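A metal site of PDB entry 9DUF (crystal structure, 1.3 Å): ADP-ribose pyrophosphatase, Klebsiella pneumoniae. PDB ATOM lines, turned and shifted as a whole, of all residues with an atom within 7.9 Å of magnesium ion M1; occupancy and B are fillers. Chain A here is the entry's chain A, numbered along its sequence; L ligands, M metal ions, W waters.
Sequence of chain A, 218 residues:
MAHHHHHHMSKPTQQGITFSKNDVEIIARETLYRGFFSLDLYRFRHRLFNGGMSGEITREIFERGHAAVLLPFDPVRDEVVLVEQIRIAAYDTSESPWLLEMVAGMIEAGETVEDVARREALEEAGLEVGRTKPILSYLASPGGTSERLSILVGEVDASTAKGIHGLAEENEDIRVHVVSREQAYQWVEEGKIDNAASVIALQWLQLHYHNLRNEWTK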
ATOM      1  N   GLN A  85      23.060  -8.802 -14.112  1.00  0.00           N
ATOM      2  CA  GLN A  85      21.920  -9.403 -13.448  1.00  0.00           C
ATOM      3  C   GLN A  85      21.704  -8.710 -12.115  1.00  0.00           C
ATOM      4  O   GLN A  85      22.605  -8.055 -11.581  1.00  0.00           O
ATOM      5  CB  GLN A  85      22.106 -10.901 -13.248  1.00  0.00           C
ATOM      6  CG  GLN A  85      23.110 -11.238 -12.207  1.00  0.00           C
ATOM      7  CD  GLN A  85      23.660 -12.625 -12.418  1.00  0.00           C
ATOM      8  OE1 GLN A  85      22.968 -13.602 -12.219  1.00  0.00           O
ATOM      9  NE2 GLN A  85      24.930 -12.713 -12.843  1.00  0.00           N
ATOM     10  N   ARG A  87      21.430  -8.277  -8.226  1.00  0.00           N
ATOM     11  CA  ARG A  87      21.984  -8.809  -6.985  1.00  0.00           C
ATOM     12  C   ARG A  87      21.354  -7.967  -5.881  1.00  0.00           C
ATOM     13  O   ARG A  87      21.838  -6.879  -5.557  1.00  0.00           O
ATOM     14  CB  ARG A  87      23.506  -8.701  -6.978  1.00  0.00           C
ATOM     15  CG  ARG A  87      24.171  -9.472  -8.068  1.00  0.00           C
ATOM     16  CD  ARG A  87      24.034 -10.949  -7.882  1.00  0.00           C
ATOM     17  NE  ARG A  87      24.843 -11.669  -8.867  1.00  0.00           N
ATOM     18  CZ  ARG A  87      24.859 -12.982  -8.999  1.00  0.00           C
ATOM     19  NH1 ARG A  87      24.110 -13.755  -8.228  1.00  0.00           N
ATOM     20  NH2 ARG A  87      25.640 -13.543  -9.915  1.00  0.00           N
ATOM     21  N   VAL A 103      31.138 -14.064 -15.456  1.00  0.00           N
ATOM     22  CA  VAL A 103      30.513 -15.374 -15.431  1.00  0.00           C
ATOM     23  C   VAL A 103      30.970 -16.083 -14.169  1.00  0.00           C
ATOM     24  O   VAL A 103      32.144 -16.034 -13.805  1.00  0.00           O
ATOM     25  CB  VAL A 103      30.995 -16.122 -16.701  1.00  0.00           C
ATOM     26  CG1 VAL A 103      30.694 -17.620 -16.621  1.00  0.00           C
ATOM     27  CG2 VAL A 103      30.370 -15.491 -17.956  1.00  0.00           C
ATOM     28  N   ALA A 104      30.044 -16.743 -13.481  1.00  0.00           N
ATOM     29  CA  ALA A 104      30.422 -17.414 -12.239  1.00  0.00           C
ATOM     30  C   ALA A 104      29.332 -18.385 -11.824  1.00  0.00           C
ATOM     31  O   ALA A 104      28.145 -18.164 -12.107  1.00  0.00           O
ATOM     32  CB  ALA A 104      30.632 -16.406 -11.107  1.00  0.00           C
ATOM     33  N   GLY A 105      29.737 -19.460 -11.143  1.00  0.00           N
ATOM     34  CA  GLY A 105      28.753 -20.364 -10.573  1.00  0.00           C
ATOM     35  C   GLY A 105      29.325 -21.179  -9.431  1.00  0.00           C
ATOM     36  O   GLY A 105      30.542 -21.247  -9.220  1.00  0.00           O
ATOM     37  N   MET A 106      28.416 -21.824  -8.696  1.00  0.00           N
ATOM     38  CA  MET A 106      28.824 -22.638  -7.567  1.00  0.00           C
ATOM     39  C   MET A 106      29.488 -23.924  -8.037  1.00  0.00           C
ATOM     40  O   MET A 106      29.093 -24.516  -9.056  1.00  0.00           O
ATOM     41  CB  MET A 106      27.623 -23.005  -6.706  1.00  0.00           C
ATOM     42  CG  MET A 106      28.023 -23.710  -5.401  1.00  0.00           C
ATOM     43  SD  MET A 106      26.661 -24.376  -4.443  1.00  0.00           S
ATOM     44  CE  MET A 106      27.549 -25.302  -3.194  1.00  0.00           C
ATOM     45  N   VAL A 116      33.166 -25.972 -14.159  1.00  0.00           N
ATOM     46  CA  VAL A 116      32.100 -25.039 -13.815  1.00  0.00           C
ATOM     47  C   VAL A 116      32.202 -23.774 -14.645  1.00  0.00           C
ATOM     48  O   VAL A 116      31.194 -23.280 -15.175  1.00  0.00           O
ATOM     49  CB  VAL A 116      32.088 -24.751 -12.303  1.00  0.00           C
ATOM     50  CG1 VAL A 116      31.048 -23.690 -11.986  1.00  0.00           C
ATOM     51  CG2 VAL A 116      31.796 -26.032 -11.534  1.00  0.00           C
ATOM     52  N   ARG A 119      30.959 -24.397 -18.200  1.00  0.00           N
ATOM     53  CA  ARG A 119      29.519 -24.572 -18.258  1.00  0.00           C
ATOM     54  C   ARG A 119      28.794 -23.235 -18.057  1.00  0.00           C
ATOM     55  O   ARG A 119      27.876 -22.898 -18.815  1.00  0.00           O
ATOM     56  CB  ARG A 119      29.071 -25.588 -17.199  1.00  0.00           C
ATOM     57  CG  ARG A 119      27.580 -25.775 -17.102  1.00  0.00           C
ATOM     58  CD  ARG A 119      27.189 -26.822 -16.054  1.00  0.00           C
ATOM     59  NE  ARG A 119      27.400 -26.371 -14.688  1.00  0.00           N
ATOM     60  CZ  ARG A 119      28.151 -27.002 -13.783  1.00  0.00           C
ATOM     61  NH1 ARG A 119      28.843 -28.090 -14.097  1.00  0.00           N
ATOM     62  NH2 ARG A 119      28.204 -26.534 -12.546  1.00  0.00           N
ATOM     63  N   GLU A 120      29.213 -22.465 -17.062  1.00  0.00           N
ATOM     64  CA  GLU A 120      28.523 -21.202 -16.799  1.00  0.00           C
ATOM     65  C   GLU A 120      28.724 -20.213 -17.936  1.00  0.00           C
ATOM     66  O   GLU A 120      27.845 -19.401 -18.215  1.00  0.00           O
ATOM     67  CB  GLU A 120      28.985 -20.607 -15.472  1.00  0.00           C
ATOM     68  CG  GLU A 120      28.663 -21.443 -14.234  1.00  0.00           C
ATOM     69  CD  GLU A 120      27.232 -21.308 -13.771  1.00  0.00           C
ATOM     70  OE1 GLU A 120      26.493 -20.420 -14.256  1.00  0.00           O
ATOM     71  OE2 GLU A 120      26.846 -22.102 -12.887  1.00  0.00           O
ATOM     72  N   ALA A 121      29.874 -20.257 -18.608  1.00  0.00           N
ATOM     73  CA  ALA A 121      30.058 -19.336 -19.722  1.00  0.00           C
ATOM     74  C   ALA A 121      29.020 -19.587 -20.803  1.00  0.00           C
ATOM     75  O   ALA A 121      28.510 -18.643 -21.409  1.00  0.00           O
ATOM     76  CB  ALA A 121      31.483 -19.449 -20.263  1.00  0.00           C
ATOM     77  N   GLU A 123      25.930 -21.121 -20.280  1.00  0.00           N
ATOM     78  CA  GLU A 123      24.595 -20.861 -19.768  1.00  0.00           C
ATOM     79  C   GLU A 123      24.315 -19.370 -19.586  1.00  0.00           C
ATOM     80  O   GLU A 123      23.177 -18.918 -19.783  1.00  0.00           O
ATOM     81  CB  GLU A 123      24.413 -21.556 -18.425  1.00  0.00           C
ATOM     82  CG  GLU A 123      24.523 -23.058 -18.440  1.00  0.00           C
ATOM     83  CD  GLU A 123      24.285 -23.658 -17.062  1.00  0.00           C
ATOM     84  OE1 GLU A 123      24.081 -22.875 -16.095  1.00  0.00           O
ATOM     85  OE2 GLU A 123      24.306 -24.891 -16.926  1.00  0.00           O
ATOM     86  N   GLU A 124      25.315 -18.598 -19.170  1.00  0.00           N
ATOM     87  CA  GLU A 124      25.094 -17.224 -18.775  1.00  0.00           C
ATOM     88  C   GLU A 124      25.368 -16.222 -19.879  1.00  0.00           C
ATOM     89  O   GLU A 124      24.869 -15.092 -19.802  1.00  0.00           O
ATOM     90  CB  GLU A 124      25.972 -16.857 -17.570  1.00  0.00           C
ATOM     91  CG  GLU A 124      25.612 -17.655 -16.348  1.00  0.00           C
ATOM     92  CD  GLU A 124      26.206 -17.136 -15.064  1.00  0.00           C
ATOM     93  OE1 GLU A 124      27.174 -16.353 -15.096  1.00  0.00           O
ATOM     94  OE2 GLU A 124      25.679 -17.517 -14.009  1.00  0.00           O
ATOM     95  N   GLY A 166      20.967 -16.936 -18.963  1.00  0.00           N
ATOM     96  CA  GLY A 166      20.581 -17.403 -17.660  1.00  0.00           C
ATOM     97  C   GLY A 166      19.390 -18.336 -17.739  1.00  0.00           C
ATOM     98  O   GLY A 166      18.608 -18.334 -18.689  1.00  0.00           O
ATOM     99  N   LEU A 167      19.273 -19.167 -16.709  1.00  0.00           N
ATOM    100  CA  LEU A 167      18.207 -20.164 -16.621  1.00  0.00           C
ATOM    101  C   LEU A 167      16.997 -19.472 -16.011  1.00  0.00           C
ATOM    102  O   LEU A 167      16.947 -19.246 -14.792  1.00  0.00           O
ATOM    103  CB  LEU A 167      18.688 -21.356 -15.807  1.00  0.00           C
ATOM    104  CG  LEU A 167      20.125 -21.808 -16.135  1.00  0.00           C
ATOM    105  CD1 LEU A 167      20.552 -22.995 -15.286  1.00  0.00           C
ATOM    106  CD2 LEU A 167      20.288 -22.125 -17.624  1.00  0.00           C
ATOM    107  N   GLU A 170      14.945 -20.786 -13.227  1.00  0.00           N
ATOM    108  CA  GLU A 170      15.596 -20.657 -11.923  1.00  0.00           C
ATOM    109  C   GLU A 170      15.705 -19.210 -11.478  1.00  0.00           C
ATOM    110  O   GLU A 170      16.423 -18.920 -10.519  1.00  0.00           O
ATOM    111  CB  GLU A 170      16.975 -21.311 -11.993  1.00  0.00           C
ATOM    112  CG  GLU A 170      16.936 -22.784 -12.390  1.00  0.00           C
ATOM    113  CD  GLU A 170      18.315 -23.392 -12.593  1.00  0.00           C
ATOM    114  OE1 GLU A 170      19.302 -22.635 -12.679  1.00  0.00           O
ATOM    115  OE2 GLU A 170      18.418 -24.636 -12.640  1.00  0.00           O
ATOM    116  N   GLU A 172      17.127 -16.685 -12.998  1.00  0.00           N
ATOM    117  CA  GLU A 172      18.447 -16.161 -13.339  1.00  0.00           C
ATOM    118  C   GLU A 172      18.312 -15.463 -14.682  1.00  0.00           C
ATOM    119  O   GLU A 172      18.340 -16.123 -15.732  1.00  0.00           O
ATOM    120  CB  GLU A 172      19.467 -17.304 -13.399  1.00  0.00           C
ATOM    121  CG  GLU A 172      20.910 -16.865 -13.594  1.00  0.00           C
ATOM    122  CD  GLU A 172      21.870 -18.036 -13.820  1.00  0.00           C
ATOM    123  OE1 GLU A 172      21.538 -18.927 -14.624  1.00  0.00           O
ATOM    124  OE2 GLU A 172      22.958 -18.076 -13.188  1.00  0.00           O
ATOM    125  N   ILE A 174      19.801 -12.779 -17.216  1.00  0.00           N
ATOM    126  CA  ILE A 174      21.147 -12.252 -17.442  1.00  0.00           C
ATOM    127  C   ILE A 174      21.211 -11.599 -18.809  1.00  0.00           C
ATOM    128  O   ILE A 174      20.718 -12.166 -19.789  1.00  0.00           O
ATOM    129  CB  ILE A 174      22.215 -13.380 -17.361  1.00  0.00           C
ATOM    130  CG1 ILE A 174      22.176 -14.031 -15.975  1.00  0.00           C
ATOM    131  CG2 ILE A 174      23.602 -12.811 -17.653  1.00  0.00           C
ATOM    132  CD1 ILE A 174      23.098 -15.250 -15.826  1.00  0.00           C
HETATM  133  N1  LIG L   1      18.139 -18.952  -2.852  1.00  0.00           N
HETATM  134  C1  LIG L   1      18.923 -17.990  -2.276  1.00  0.00           C
HETATM  135  O1  LIG L   1      18.634 -17.574  -1.179  1.00  0.00           O
HETATM  136  N2  LIG L   1      20.037 -17.487  -2.916  1.00  0.00           N
HETATM  137  C2  LIG L   1      20.386 -17.920  -4.161  1.00  0.00           C
HETATM  138  O2  LIG L   1      21.383 -17.432  -4.669  1.00  0.00           O
HETATM  139  C3  LIG L   1      19.608 -18.904  -4.753  1.00  0.00           C
HETATM  140  N3  LIG L   1      19.925 -19.386  -5.992  1.00  0.00           N
HETATM  141  C4  LIG L   1      19.121 -20.365  -6.541  1.00  0.00           C
HETATM  142  C5  LIG L   1      19.460 -20.828  -7.785  1.00  0.00           C
HETATM  143  C6  LIG L   1      18.698 -21.814  -8.394  1.00  0.00           C
HETATM  144  C7  LIG L   1      19.145 -22.279  -9.740  1.00  0.00           C
HETATM  145  C8  LIG L   1      17.578 -22.334  -7.733  1.00  0.00           C
HETATM  146  C9  LIG L   1      16.713 -23.400  -8.345  1.00  0.00           C
HETATM  147  C10 LIG L   1      17.242 -21.849  -6.468  1.00  0.00           C
HETATM  148  C11 LIG L   1      18.007 -20.874  -5.868  1.00  0.00           C
HETATM  149  N4  LIG L   1      17.668 -20.382  -4.627  1.00  0.00           N
HETATM  150  C12 LIG L   1      18.484 -19.414  -4.084  1.00  0.00           C
HETATM  151  C13 LIG L   1      16.501 -20.896  -3.823  1.00  0.00           C
HETATM  152  C14 LIG L   1      15.136 -20.323  -4.205  1.00  0.00           C
HETATM  153  O3  LIG L   1      15.061 -18.969  -3.801  1.00  0.00           O
HETATM  154  C15 LIG L   1      14.005 -21.072  -3.522  1.00  0.00           C
HETATM  155  O4  LIG L   1      14.181 -20.978  -2.117  1.00  0.00           O
HETATM  156  C16 LIG L   1      13.940 -22.546  -3.938  1.00  0.00           C
HETATM  157  O5  LIG L   1      14.036 -22.631  -5.338  1.00  0.00           O
HETATM  158  C17 LIG L   1      12.669 -23.225  -3.446  1.00  0.00           C
HETATM  159  O6  LIG L   1      11.534 -22.543  -3.923  1.00  0.00           O
HETATM  160  P1  LIG L   1      10.056 -22.992  -3.463  1.00  0.00           P
HETATM  161  O7  LIG L   1      10.011 -22.975  -1.954  1.00  0.00           O
HETATM  162  O8  LIG L   1       9.768 -24.384  -3.974  1.00  0.00           O
HETATM  163  O9  LIG L   1       9.037 -22.016  -3.999  1.00  0.00           O
HETATM  164 MG    MG M   1      24.702 -19.302 -13.485  1.00  0.00          MG
HETATM  165 MG    MG M   2      27.240 -14.647 -12.946  1.00  0.00          MG
HETATM  166  O   HOH W   1      23.781 -20.176 -15.187  1.00  0.00           O
HETATM  167  O   HOH W   2      23.811 -21.003 -12.656  1.00  0.00           O
HETATM  168  O   HOH W   3      25.475 -18.981 -11.706  1.00  0.00           O
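OE1 of Glu 124 lies within hydrogen-bond range of N of Ala 104, 3.3 Å away. OE1 of Glu 172 sits at hydrogen-bond distance from N of Leu 167 (3.1 Å).
Magnesium ion M1 is bound by water W3, at 2.0 Å. Water W2 binds magnesium ion M1 (2.1 Å). OE2 of Glu 124 binds magnesium ion M1 (2.1 Å). Water W1 is bound to magnesium ion M1 (2.1 Å). The side-chain carboxylate (OE2) of Glu 172 is bound to magnesium ion M1 (2.2 Å). The side-chain carboxylate (OE1) of Glu 120 binds magnesium ion M1, at 2.2 Å.
Water W1 bridges the side-chain carboxylate (OE1) of Glu 172 (2.6 Å) and the side-chain carboxylate (OE1) of Glu 123 (2.9 Å).
O of Ala 104 touches magnesium ion M1, at 3.9 Å. Four residues have an atom within 4 Å of magnesium ion M1: Ala 104, Glu 120, Glu 124 and Glu 172.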
